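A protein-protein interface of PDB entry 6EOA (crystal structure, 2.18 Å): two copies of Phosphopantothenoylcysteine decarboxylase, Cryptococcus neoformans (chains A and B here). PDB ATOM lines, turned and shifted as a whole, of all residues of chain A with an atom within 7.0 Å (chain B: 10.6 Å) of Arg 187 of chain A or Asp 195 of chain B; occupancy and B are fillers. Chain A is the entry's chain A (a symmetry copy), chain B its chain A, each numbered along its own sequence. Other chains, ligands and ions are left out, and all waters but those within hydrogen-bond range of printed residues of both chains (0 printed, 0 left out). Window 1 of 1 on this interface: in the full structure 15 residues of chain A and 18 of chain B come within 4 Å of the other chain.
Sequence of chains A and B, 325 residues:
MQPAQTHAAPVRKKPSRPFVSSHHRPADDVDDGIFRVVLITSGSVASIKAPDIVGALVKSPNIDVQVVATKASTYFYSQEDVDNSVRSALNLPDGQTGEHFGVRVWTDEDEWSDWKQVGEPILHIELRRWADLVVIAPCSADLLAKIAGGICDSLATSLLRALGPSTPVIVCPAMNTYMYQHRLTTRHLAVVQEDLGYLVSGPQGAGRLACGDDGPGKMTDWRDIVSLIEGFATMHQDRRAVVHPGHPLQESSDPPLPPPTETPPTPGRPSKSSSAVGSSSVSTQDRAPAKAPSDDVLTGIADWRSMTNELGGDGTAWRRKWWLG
Among the printed residues, merely in contact across the chains: His 182 of chain A with Arg 161 of chain B (3.5 Å), His 182 of chain A with Leu 196 of chain B (3.5 Å), Arg 183 of chain A with Glu 194 of chain B (3.6 Å), Leu 184 of chain A with Ile 147 of chain B (3.5 Å), Leu 184 of chain A with Ala 148 of chain B (3.7 Å), Leu 184 of chain A with Gly 150 of chain B (3.5 Å) and His 188 of chain A with Arg 161 of chain B (3.9 Å).
Hydrophobic or aromatic side chains of chain B that line the printed part of chain A: Leu 196. Hydrophobic or aromatic side chains of chain A that line the printed part of chain B: His 182, Leu 184 and His 188. Among the printed residues, Asp or Glu carboxylates within 4 Å of a Lys or Arg side-chain nitrogen of the other chain: Arg 187 of chain A with Asp 195 of chain B (2.7 Å).
Printed residues of chain B within 4 Å of His 182 of chain A: Arg 161 and Leu 196. Of chain B, only Ile 147 (3.5 Å), Ala 148 (3.7 Å) and Gly 150 (3.5 Å) come within 4 Å of Leu 184 of chain A. Of the printed residues of chain B, Thr 185 of chain A touches Arg 161. Arg 187 of chain A touches just one residue of chain B: Asp 195 (2.7 Å). Of chain B, only Gly 149 (3.1 Å) and Arg 161 (3.9 Å) come within 4 Å of His 188 of chain A. No residue of chain B comes within 4 Å of Ala 190 of chain A. No residue of chain B comes within 4 Å of Val 191 of chain A. Of the printed residues of chain A, Gly 149 of chain B touches His 188. Of the printed residues of chain A, Gly 150 of chain B touches Leu 184. Arg 187 of chain B touches none of the printed residues of chain A. Ala 190 of chain B touches none of the printed residues of chain A. Printed residues of chain A within 4 Å of Glu 194 of chain B: Arg 183. Asp 195 of chain B touches just these residues of chain A: Arg 183 (3.1 Å) and Arg 187 (2.7 Å). The nearest residue of chain B that does not touch Arg 187 of chain A is Val 191 of chain B (4.5 Å).
Positions printed for both chains: 148, 186, 187, 188, 189, 190, 191 and 192. Of the 11 pairs that touch across the chains among the printed residues, none has its exchanged pair printed and touching as well.
A ring nitrogen (NE2) of His 188 of chain A lies close to the backbone carbonyl oxygen (O) of Gly 149 of chain B (3.3 Å). The guanidinium group (NH1) of Arg 161 of chain B lies within hydrogen-bond range of the side-chain hydroxyl (OG1) of Thr 185 of chain A, 2.9 Å away. NH1 of Arg 183 of chain A is in hydrogen-bond range of O of Asp 195 of chain B (3.1 Å). The guanidinium group of Arg 187 of chain A is in salt-bridge range of the side-chain carboxylate of Asp 195 of chain B (2.7 Å).
O of Gly 150 of chain B is in hydrogen-bond range of NE of Arg 161 of chain B, 3.2 Å away. The backbone carbonyl oxygen of Val 191 of chain B sits at hydrogen-bond distance from the backbone NH of Leu 196 of chain B. A ring nitrogen (ND1) of His 182 of chain A sits close to the backbone NH (N) of Leu 184 of chain A (3.2 Å). The backbone carbonyl oxygen (O) of Arg 183 of chain A lies within hydrogen-bond range of the side-chain hydroxyl (OG1) of Thr 186 of chain A, 3.2 Å away. ND1 of His 188 of chain A lies close to O of Leu 184 of chain A.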
ATOM      1  N   LEU A 144     -33.347  24.266 -18.914  1.00  0.00           N
ATOM      2  CA  LEU A 144     -34.307  23.234 -18.546  1.00  0.00           C
ATOM      3  C   LEU A 144     -34.230  22.940 -17.051  1.00  0.00           C
ATOM      4  O   LEU A 144     -35.252  22.857 -16.370  1.00  0.00           O
ATOM      5  CB  LEU A 144     -34.060  21.955 -19.353  1.00  0.00           C
ATOM      6  CG  LEU A 144     -34.896  20.751 -18.915  1.00  0.00           C
ATOM      7  CD1 LEU A 144     -36.385  21.041 -19.068  1.00  0.00           C
ATOM      8  CD2 LEU A 144     -34.505  19.496 -19.687  1.00  0.00           C
ATOM      9  N   ALA A 148     -37.108  23.792 -14.270  1.00  0.00           N
ATOM     10  CA  ALA A 148     -37.590  22.717 -13.412  1.00  0.00           C
ATOM     11  C   ALA A 148     -37.320  23.033 -11.948  1.00  0.00           C
ATOM     12  O   ALA A 148     -38.072  22.622 -11.067  1.00  0.00           O
ATOM     13  CB  ALA A 148     -36.942  21.398 -13.797  1.00  0.00           C
ATOM     14  N   HIS A 182     -28.502  12.138 -19.954  1.00  0.00           N
ATOM     15  CA  HIS A 182     -28.301  12.284 -18.514  1.00  0.00           C
ATOM     16  C   HIS A 182     -29.602  11.997 -17.760  1.00  0.00           C
ATOM     17  O   HIS A 182     -30.689  12.321 -18.238  1.00  0.00           O
ATOM     18  CB  HIS A 182     -27.786  13.693 -18.198  1.00  0.00           C
ATOM     19  CG  HIS A 182     -27.212  13.846 -16.826  1.00  0.00           C
ATOM     20  ND1 HIS A 182     -27.978  14.173 -15.727  1.00  0.00           N
ATOM     21  CD2 HIS A 182     -25.938  13.746 -16.377  1.00  0.00           C
ATOM     22  CE1 HIS A 182     -27.203  14.257 -14.663  1.00  0.00           C
ATOM     23  NE2 HIS A 182     -25.959  14.003 -15.029  1.00  0.00           N
ATOM     24  N   ARG A 183     -29.481  11.386 -16.587  1.00  0.00           N
ATOM     25  CA  ARG A 183     -30.641  10.942 -15.823  1.00  0.00           C
ATOM     26  C   ARG A 183     -31.578  12.082 -15.440  1.00  0.00           C
ATOM     27  O   ARG A 183     -32.794  11.887 -15.331  1.00  0.00           O
ATOM     28  CB  ARG A 183     -30.191  10.209 -14.559  1.00  0.00           C
ATOM     29  CG  ARG A 183     -31.295   9.419 -13.874  1.00  0.00           C
ATOM     30  CD  ARG A 183     -30.861   7.979 -13.656  1.00  0.00           C
ATOM     31  NE  ARG A 183     -31.862   7.194 -12.940  1.00  0.00           N
ATOM     32  CZ  ARG A 183     -31.573   6.277 -12.022  1.00  0.00           C
ATOM     33  NH1 ARG A 183     -30.309   6.032 -11.703  1.00  0.00           N
ATOM     34  NH2 ARG A 183     -32.547   5.606 -11.420  1.00  0.00           N
ATOM     35  N   LEU A 184     -31.014  13.270 -15.242  1.00  0.00           N
ATOM     36  CA  LEU A 184     -31.783  14.404 -14.746  1.00  0.00           C
ATOM     37  C   LEU A 184     -32.597  15.089 -15.836  1.00  0.00           C
ATOM     38  O   LEU A 184     -33.520  15.849 -15.542  1.00  0.00           O
ATOM     39  CB  LEU A 184     -30.852  15.415 -14.084  1.00  0.00           C
ATOM     40  CG  LEU A 184     -30.116  14.880 -12.854  1.00  0.00           C
ATOM     41  CD1 LEU A 184     -29.216  15.939 -12.262  1.00  0.00           C
ATOM     42  CD2 LEU A 184     -31.114  14.381 -11.820  1.00  0.00           C
ATOM     43  N   THR A 185     -32.251  14.825 -17.090  1.00  0.00           N
ATOM     44  CA  THR A 185     -32.964  15.415 -18.216  1.00  0.00           C
ATOM     45  C   THR A 185     -34.424  14.979 -18.241  1.00  0.00           C
ATOM     46  O   THR A 185     -35.330  15.806 -18.343  1.00  0.00           O
ATOM     47  CB  THR A 185     -32.309  15.037 -19.550  1.00  0.00           C
ATOM     48  OG1 THR A 185     -31.003  15.619 -19.621  1.00  0.00           O
ATOM     49  CG2 THR A 185     -33.151  15.541 -20.719  1.00  0.00           C
ATOM     50  N   THR A 186     -34.645  13.674 -18.142  1.00  0.00           N
ATOM     51  CA  THR A 186     -35.991  13.122 -18.194  1.00  0.00           C
ATOM     52  C   THR A 186     -36.805  13.513 -16.964  1.00  0.00           C
ATOM     53  O   THR A 186     -38.018  13.682 -17.045  1.00  0.00           O
ATOM     54  CB  THR A 186     -35.957  11.592 -18.316  1.00  0.00           C
ATOM     55  OG1 THR A 186     -35.216  11.041 -17.221  1.00  0.00           O
ATOM     56  CG2 THR A 186     -35.290  11.187 -19.621  1.00  0.00           C
ATOM     57  N   ARG A 187     -36.134  13.654 -15.825  1.00  0.00           N
ATOM     58  CA  ARG A 187     -36.796  14.110 -14.607  1.00  0.00           C
ATOM     59  C   ARG A 187     -37.218  15.580 -14.719  1.00  0.00           C
ATOM     60  O   ARG A 187     -38.234  15.984 -14.151  1.00  0.00           O
ATOM     61  CB  ARG A 187     -35.884  13.912 -13.395  1.00  0.00           C
ATOM     62  CG  ARG A 187     -36.479  14.396 -12.080  1.00  0.00           C
ATOM     63  CD  ARG A 187     -35.545  14.131 -10.906  1.00  0.00           C
ATOM     64  NE  ARG A 187     -35.384  12.703 -10.646  1.00  0.00           N
ATOM     65  CZ  ARG A 187     -34.512  12.190  -9.782  1.00  0.00           C
ATOM     66  NH1 ARG A 187     -33.707  12.987  -9.088  1.00  0.00           N
ATOM     67  NH2 ARG A 187     -34.442  10.877  -9.615  1.00  0.00           N
ATOM     68  N   HIS A 188     -36.442  16.376 -15.450  1.00  0.00           N
ATOM     69  CA  HIS A 188     -36.767  17.790 -15.644  1.00  0.00           C
ATOM     70  C   HIS A 188     -37.832  17.970 -16.719  1.00  0.00           C
ATOM     71  O   HIS A 188     -38.703  18.837 -16.600  1.00  0.00           O
ATOM     72  CB  HIS A 188     -35.518  18.595 -16.005  1.00  0.00           C
ATOM     73  CG  HIS A 188     -34.505  18.667 -14.905  1.00  0.00           C
ATOM     74  ND1 HIS A 188     -33.224  19.138 -15.100  1.00  0.00           N
ATOM     75  CD2 HIS A 188     -34.583  18.318 -13.598  1.00  0.00           C
ATOM     76  CE1 HIS A 188     -32.558  19.078 -13.961  1.00  0.00           C
ATOM     77  NE2 HIS A 188     -33.360  18.587 -13.033  1.00  0.00           N
ATOM     78  N   LEU A 189     -37.757  17.158 -17.771  1.00  0.00           N
ATOM     79  CA  LEU A 189     -38.792  17.154 -18.796  1.00  0.00           C
ATOM     80  C   LEU A 189     -40.121  16.767 -18.167  1.00  0.00           C
ATOM     81  O   LEU A 189     -41.166  17.287 -18.542  1.00  0.00           O
ATOM     82  CB  LEU A 189     -38.446  16.192 -19.938  1.00  0.00           C
ATOM     83  CG  LEU A 189     -37.273  16.546 -20.856  1.00  0.00           C
ATOM     84  CD1 LEU A 189     -37.036  15.419 -21.861  1.00  0.00           C
ATOM     85  CD2 LEU A 189     -37.512  17.870 -21.575  1.00  0.00           C
ATOM     86  N   ALA A 190     -40.068  15.855 -17.202  1.00  0.00           N
ATOM     87  CA  ALA A 190     -41.260  15.407 -16.492  1.00  0.00           C
ATOM     88  C   ALA A 190     -41.875  16.538 -15.673  1.00  0.00           C
ATOM     89  O   ALA A 190     -43.079  16.782 -15.747  1.00  0.00           O
ATOM     90  CB  ALA A 190     -40.930  14.222 -15.594  1.00  0.00           C
ATOM     91  N   VAL A 191     -41.042  17.220 -14.889  1.00  0.00           N
ATOM     92  CA  VAL A 191     -41.481  18.368 -14.104  1.00  0.00           C
ATOM     93  C   VAL A 191     -42.052  19.458 -15.008  1.00  0.00           C
ATOM     94  O   VAL A 191     -43.142  19.974 -14.779  1.00  0.00           O
ATOM     95  CB  VAL A 191     -40.323  18.952 -13.264  1.00  0.00           C
ATOM     96  CG1 VAL A 191     -40.702  20.313 -12.698  1.00  0.00           C
ATOM     97  CG2 VAL A 191     -39.937  17.993 -12.154  1.00  0.00           C
ATOM     98  N   VAL A 192     -41.308  19.792 -16.053  1.00  0.00           N
ATOM     99  CA  VAL A 192     -41.715  20.823 -16.996  1.00  0.00           C
ATOM    100  C   VAL A 192     -43.046  20.482 -17.695  1.00  0.00           C
ATOM    101  O   VAL A 192     -43.873  21.365 -17.950  1.00  0.00           O
ATOM    102  CB  VAL A 192     -40.585  21.047 -18.030  1.00  0.00           C
ATOM    103  CG1 VAL A 192     -41.111  21.636 -19.313  1.00  0.00           C
ATOM    104  CG2 VAL A 192     -39.502  21.934 -17.427  1.00  0.00           C
ATOM    105  N   ALA B 145     -24.993  20.862  -4.704  1.00  0.00           N
ATOM    106  CA  ALA B 145     -26.375  21.249  -4.968  1.00  0.00           C
ATOM    107  C   ALA B 145     -26.621  21.460  -6.463  1.00  0.00           C
ATOM    108  O   ALA B 145     -27.650  21.042  -6.992  1.00  0.00           O
ATOM    109  CB  ALA B 145     -26.729  22.511  -4.187  1.00  0.00           C
ATOM    110  N   ILE B 147     -24.913  20.119  -8.986  1.00  0.00           N
ATOM    111  CA  ILE B 147     -24.831  18.809  -9.626  1.00  0.00           C
ATOM    112  C   ILE B 147     -26.133  18.037  -9.437  1.00  0.00           C
ATOM    113  O   ILE B 147     -26.689  17.492 -10.395  1.00  0.00           O
ATOM    114  CB  ILE B 147     -23.659  17.975  -9.068  1.00  0.00           C
ATOM    115  CG1 ILE B 147     -22.322  18.593  -9.479  1.00  0.00           C
ATOM    116  CG2 ILE B 147     -23.742  16.534  -9.562  1.00  0.00           C
ATOM    117  CD1 ILE B 147     -21.126  18.017  -8.749  1.00  0.00           C
ATOM    118  N   ALA B 148     -26.616  18.004  -8.199  1.00  0.00           N
ATOM    119  CA  ALA B 148     -27.861  17.317  -7.873  1.00  0.00           C
ATOM    120  C   ALA B 148     -29.038  17.967  -8.587  1.00  0.00           C
ATOM    121  O   ALA B 148     -30.012  17.299  -8.926  1.00  0.00           O
ATOM    122  CB  ALA B 148     -28.088  17.312  -6.371  1.00  0.00           C
ATOM    123  N   GLY B 149     -28.940  19.271  -8.818  1.00  0.00           N
ATOM    124  CA  GLY B 149     -29.994  20.005  -9.491  1.00  0.00           C
ATOM    125  C   GLY B 149     -29.920  19.945 -11.006  1.00  0.00           C
ATOM    126  O   GLY B 149     -30.873  20.307 -11.691  1.00  0.00           O
ATOM    127  N   GLY B 150     -28.787  19.490 -11.536  1.00  0.00           N
ATOM    128  CA  GLY B 150     -28.622  19.364 -12.974  1.00  0.00           C
ATOM    129  C   GLY B 150     -28.267  20.677 -13.642  1.00  0.00           C
ATOM    130  O   GLY B 150     -28.272  20.787 -14.868  1.00  0.00           O
ATOM    131  N   LEU B 160     -19.455  17.746 -16.235  1.00  0.00           N
ATOM    132  CA  LEU B 160     -20.104  16.659 -15.504  1.00  0.00           C
ATOM    133  C   LEU B 160     -21.414  16.235 -16.164  1.00  0.00           C
ATOM    134  O   LEU B 160     -21.709  15.046 -16.263  1.00  0.00           O
ATOM    135  CB  LEU B 160     -20.353  17.072 -14.052  1.00  0.00           C
ATOM    136  CG  LEU B 160     -19.109  17.089 -13.160  1.00  0.00           C
ATOM    137  CD1 LEU B 160     -19.330  17.958 -11.934  1.00  0.00           C
ATOM    138  CD2 LEU B 160     -18.733  15.677 -12.752  1.00  0.00           C
ATOM    139  N   ARG B 161     -22.188  17.216 -16.623  1.00  0.00           N
ATOM    140  CA  ARG B 161     -23.473  16.948 -17.262  1.00  0.00           C
ATOM    141  C   ARG B 161     -23.293  16.225 -18.594  1.00  0.00           C
ATOM    142  O   ARG B 161     -24.153  15.451 -19.006  1.00  0.00           O
ATOM    143  CB  ARG B 161     -24.243  18.252 -17.478  1.00  0.00           C
ATOM    144  CG  ARG B 161     -25.696  18.070 -17.897  1.00  0.00           C
ATOM    145  CD  ARG B 161     -26.546  17.530 -16.750  1.00  0.00           C
ATOM    146  NE  ARG B 161     -27.835  18.216 -16.654  1.00  0.00           N
ATOM    147  CZ  ARG B 161     -28.872  17.965 -17.444  1.00  0.00           C
ATOM    148  NH1 ARG B 161     -28.772  17.044 -18.392  1.00  0.00           N
ATOM    149  NH2 ARG B 161     -30.007  18.635 -17.290  1.00  0.00           N
ATOM    150  N   PRO B 165     -21.437   7.402 -19.223  1.00  0.00           N
ATOM    151  CA  PRO B 165     -21.357   6.477 -18.085  1.00  0.00           C
ATOM    152  C   PRO B 165     -20.047   5.691 -18.088  1.00  0.00           C
ATOM    153  O   PRO B 165     -19.730   4.998 -17.120  1.00  0.00           O
ATOM    154  CB  PRO B 165     -22.555   5.548 -18.299  1.00  0.00           C
ATOM    155  CG  PRO B 165     -22.815   5.600 -19.764  1.00  0.00           C
ATOM    156  CD  PRO B 165     -22.468   6.998 -20.194  1.00  0.00           C
ATOM    157  N   VAL B 169     -16.836   9.006 -11.585  1.00  0.00           N
ATOM    158  CA  VAL B 169     -16.711  10.293 -10.917  1.00  0.00           C
ATOM    159  C   VAL B 169     -16.522  10.110  -9.420  1.00  0.00           C
ATOM    160  O   VAL B 169     -17.286   9.391  -8.777  1.00  0.00           O
ATOM    161  CB  VAL B 169     -17.947  11.188 -11.152  1.00  0.00           C
ATOM    162  CG1 VAL B 169     -17.839  12.474 -10.340  1.00  0.00           C
ATOM    163  CG2 VAL B 169     -18.108  11.496 -12.628  1.00  0.00           C
ATOM    164  N   THR B 186     -27.554  15.539   2.595  1.00  0.00           N
ATOM    165  CA  THR B 186     -27.754  14.102   2.478  1.00  0.00           C
ATOM    166  C   THR B 186     -28.692  13.758   1.324  1.00  0.00           C
ATOM    167  O   THR B 186     -28.549  12.715   0.691  1.00  0.00           O
ATOM    168  CB  THR B 186     -28.313  13.513   3.781  1.00  0.00           C
ATOM    169  OG1 THR B 186     -29.537  14.178   4.118  1.00  0.00           O
ATOM    170  CG2 THR B 186     -27.315  13.704   4.911  1.00  0.00           C
ATOM    171  N   ARG B 187     -29.651  14.637   1.054  1.00  0.00           N
ATOM    172  CA  ARG B 187     -30.549  14.453  -0.081  1.00  0.00           C
ATOM    173  C   ARG B 187     -29.807  14.623  -1.413  1.00  0.00           C
ATOM    174  O   ARG B 187     -30.145  13.975  -2.404  1.00  0.00           O
ATOM    175  CB  ARG B 187     -31.722  15.431  -0.001  1.00  0.00           C
ATOM    176  CG  ARG B 187     -32.695  15.338  -1.168  1.00  0.00           C
ATOM    177  CD  ARG B 187     -33.863  16.303  -1.009  1.00  0.00           C
ATOM    178  NE  ARG B 187     -34.721  15.943   0.116  1.00  0.00           N
ATOM    179  CZ  ARG B 187     -35.720  16.695   0.571  1.00  0.00           C
ATOM    180  NH1 ARG B 187     -35.992  17.864   0.002  1.00  0.00           N
ATOM    181  NH2 ARG B 187     -36.445  16.280   1.601  1.00  0.00           N
ATOM    182  N   HIS B 188     -28.798  15.491  -1.434  1.00  0.00           N
ATOM    183  CA  HIS B 188     -28.007  15.711  -2.645  1.00  0.00           C
ATOM    184  C   HIS B 188     -26.965  14.614  -2.831  1.00  0.00           C
ATOM    185  O   HIS B 188     -26.696  14.190  -3.959  1.00  0.00           O
ATOM    186  CB  HIS B 188     -27.325  17.079  -2.613  1.00  0.00           C
ATOM    187  CG  HIS B 188     -28.278  18.231  -2.663  1.00  0.00           C
ATOM    188  ND1 HIS B 188     -27.893  19.531  -2.413  1.00  0.00           N
ATOM    189  CD2 HIS B 188     -29.607  18.278  -2.928  1.00  0.00           C
ATOM    190  CE1 HIS B 188     -28.941  20.329  -2.523  1.00  0.00           C
ATOM    191  NE2 HIS B 188     -29.992  19.593  -2.837  1.00  0.00           N
ATOM    192  N   LEU B 189     -26.374  14.163  -1.728  1.00  0.00           N
ATOM    193  CA  LEU B 189     -25.458  13.031  -1.771  1.00  0.00           C
ATOM    194  C   LEU B 189     -26.198  11.804  -2.281  1.00  0.00           C
ATOM    195  O   LEU B 189     -25.637  10.992  -3.009  1.00  0.00           O
ATOM    196  CB  LEU B 189     -24.851  12.747  -0.392  1.00  0.00           C
ATOM    197  CG  LEU B 189     -23.866  13.765   0.190  1.00  0.00           C
ATOM    198  CD1 LEU B 189     -23.455  13.345   1.602  1.00  0.00           C
ATOM    199  CD2 LEU B 189     -22.641  13.926  -0.704  1.00  0.00           C
ATOM    200  N   ALA B 190     -27.465  11.684  -1.897  1.00  0.00           N
ATOM    201  CA  ALA B 190     -28.304  10.572  -2.332  1.00  0.00           C
ATOM    202  C   ALA B 190     -28.548  10.617  -3.838  1.00  0.00           C
ATOM    203  O   ALA B 190     -28.378   9.613  -4.529  1.00  0.00           O
ATOM    204  CB  ALA B 190     -29.629  10.582  -1.580  1.00  0.00           C
ATOM    205  N   VAL B 191     -28.951  11.784  -4.335  1.00  0.00           N
ATOM    206  CA  VAL B 191     -29.156  11.987  -5.766  1.00  0.00           C
ATOM    207  C   VAL B 191     -27.867  11.722  -6.542  1.00  0.00           C
ATOM    208  O   VAL B 191     -27.852  10.985  -7.525  1.00  0.00           O
ATOM    209  CB  VAL B 191     -29.650  13.419  -6.066  1.00  0.00           C
ATOM    210  CG1 VAL B 191     -29.566  13.716  -7.556  1.00  0.00           C
ATOM    211  CG2 VAL B 191     -31.068  13.608  -5.557  1.00  0.00           C
ATOM    212  N   VAL B 192     -26.780  12.320  -6.079  1.00  0.00           N
ATOM    213  CA  VAL B 192     -25.482  12.172  -6.721  1.00  0.00           C
ATOM    214  C   VAL B 192     -25.007  10.707  -6.749  1.00  0.00           C
ATOM    215  O   VAL B 192     -24.395  10.256  -7.724  1.00  0.00           O
ATOM    216  CB  VAL B 192     -24.450  13.078  -6.007  1.00  0.00           C
ATOM    217  CG1 VAL B 192     -23.041  12.586  -6.208  1.00  0.00           C
ATOM    218  CG2 VAL B 192     -24.600  14.515  -6.491  1.00  0.00           C
ATOM    219  N   GLN B 193     -25.331   9.956  -5.700  1.00  0.00           N
ATOM    220  CA  GLN B 193     -24.860   8.575  -5.565  1.00  0.00           C
ATOM    221  C   GLN B 193     -25.723   7.557  -6.304  1.00  0.00           C
ATOM    222  O   GLN B 193     -25.247   6.831  -7.170  1.00  0.00           O
ATOM    223  CB  GLN B 193     -24.785   8.187  -4.085  1.00  0.00           C
ATOM    224  CG  GLN B 193     -23.375   8.034  -3.566  1.00  0.00           C
ATOM    225  CD  GLN B 193     -23.324   7.789  -2.069  1.00  0.00           C
ATOM    226  OE1 GLN B 193     -23.881   8.558  -1.281  1.00  0.00           O
ATOM    227  NE2 GLN B 193     -22.671   6.702  -1.670  1.00  0.00           N
ATOM    228  N   GLU B 194     -26.994   7.496  -5.932  1.00  0.00           N
ATOM    229  CA  GLU B 194     -27.916   6.516  -6.491  1.00  0.00           C
ATOM    230  C   GLU B 194     -28.278   6.819  -7.939  1.00  0.00           C
ATOM    231  O   GLU B 194     -28.230   5.928  -8.795  1.00  0.00           O
ATOM    232  CB  GLU B 194     -29.192   6.431  -5.651  1.00  0.00           C
ATOM    233  CG  GLU B 194     -28.952   5.917  -4.243  1.00  0.00           C
ATOM    234  CD  GLU B 194     -29.994   6.408  -3.239  1.00  0.00           C
ATOM    235  OE1 GLU B 194     -31.053   6.942  -3.660  1.00  0.00           O
ATOM    236  OE2 GLU B 194     -29.751   6.247  -2.020  1.00  0.00           O
ATOM    237  N   ASP B 195     -28.644   8.069  -8.210  1.00  0.00           N
ATOM    238  CA  ASP B 195     -29.111   8.450  -9.537  1.00  0.00           C
ATOM    239  C   ASP B 195     -27.970   8.582 -10.548  1.00  0.00           C
ATOM    240  O   ASP B 195     -28.085   8.123 -11.681  1.00  0.00           O
ATOM    241  CB  ASP B 195     -29.887   9.767  -9.465  1.00  0.00           C
ATOM    242  CG  ASP B 195     -31.174   9.655  -8.666  1.00  0.00           C
ATOM    243  OD1 ASP B 195     -31.408   8.594  -8.054  1.00  0.00           O
ATOM    244  OD2 ASP B 195     -31.950  10.639  -8.651  1.00  0.00           O
ATOM    245  N   LEU B 196     -26.873   9.210 -10.138  1.00  0.00           N
ATOM    246  CA  LEU B 196     -25.802   9.539 -11.074  1.00  0.00           C
ATOM    247  C   LEU B 196     -24.646   8.541 -11.037  1.00  0.00           C
ATOM    248  O   LEU B 196     -23.804   8.529 -11.934  1.00  0.00           O
ATOM    249  CB  LEU B 196     -25.280  10.947 -10.798  1.00  0.00           C
ATOM    250  CG  LEU B 196     -26.327  12.063 -10.825  1.00  0.00           C
ATOM    251  CD1 LEU B 196     -25.657  13.426 -10.828  1.00  0.00           C
ATOM    252  CD2 LEU B 196     -27.240  11.914 -12.031  1.00  0.00           C
ATOM    253  N   GLY B 197     -24.601   7.711 -10.001  1.00  0.00           N
ATOM    254  CA  GLY B 197     -23.564   6.702  -9.890  1.00  0.00           C
ATOM    255  C   GLY B 197     -22.208   7.266  -9.515  1.00  0.00           C
ATOM    256  O   GLY B 197     -21.188   6.604  -9.690  1.00  0.00           O
ATOM    257  N   TYR B 198     -22.187   8.491  -9.000  1.00  0.00           N
ATOM    258  CA  TYR B 198     -20.932   9.088  -8.551  1.00  0.00           C
ATOM    259  C   TYR B 198     -20.454   8.408  -7.268  1.00  0.00           C
ATOM    260  O   TYR B 198     -21.261   7.999  -6.433  1.00  0.00           O
ATOM    261  CB  TYR B 198     -21.076  10.595  -8.303  1.00  0.00           C
ATOM    262  CG  TYR B 198     -21.355  11.457  -9.522  1.00  0.00           C
ATOM    263  CD1 TYR B 198     -21.617  10.893 -10.766  1.00  0.00           C
ATOM    264  CD2 TYR B 198     -21.346  12.846  -9.422  1.00  0.00           C
ATOM    265  CE1 TYR B 198     -21.873  11.687 -11.872  1.00  0.00           C
ATOM    266  CE2 TYR B 198     -21.598  13.648 -10.522  1.00  0.00           C
ATOM    267  CZ  TYR B 198     -21.862  13.063 -11.745  1.00  0.00           C
ATOM    268  OH  TYR B 198     -22.109  13.852 -12.844  1.00  0.00           O
ATOM    269  N   LEU B 199     -19.140   8.295  -7.114  1.00  0.00           N
ATOM    270  CA  LEU B 199     -18.559   7.762  -5.888  1.00  0.00           C
ATOM    271  C   LEU B 199     -18.243   8.893  -4.922  1.00  0.00           C
ATOM    272  O   LEU B 199     -17.648   9.900  -5.308  1.00  0.00           O
ATOM    273  CB  LEU B 199     -17.296   6.960  -6.191  1.00  0.00           C
ATOM    274  CG  LEU B 199     -17.492   5.639  -6.926  1.00  0.00           C
ATOM    275  CD1 LEU B 199     -16.147   4.976  -7.141  1.00  0.00           C
ATOM    276  CD2 LEU B 199     -18.428   4.722  -6.153  1.00  0.00           C
ATOM    277  N   VAL B 200     -18.641   8.729  -3.667  1.00  0.00           N
ATOM    278  CA  VAL B 200     -18.424   9.774  -2.677  1.00  0.00           C
ATOM    279  C   VAL B 200     -17.340   9.387  -1.690  1.00  0.00           C
ATOM    280  O   VAL B 200     -17.536   8.511  -0.850  1.00  0.00           O
ATOM    281  CB  VAL B 200     -19.711  10.099  -1.890  1.00  0.00           C
ATOM    282  CG1 VAL B 200     -19.454  11.225  -0.892  1.00  0.00           C
ATOM    283  CG2 VAL B 200     -20.832  10.471  -2.837  1.00  0.00           C
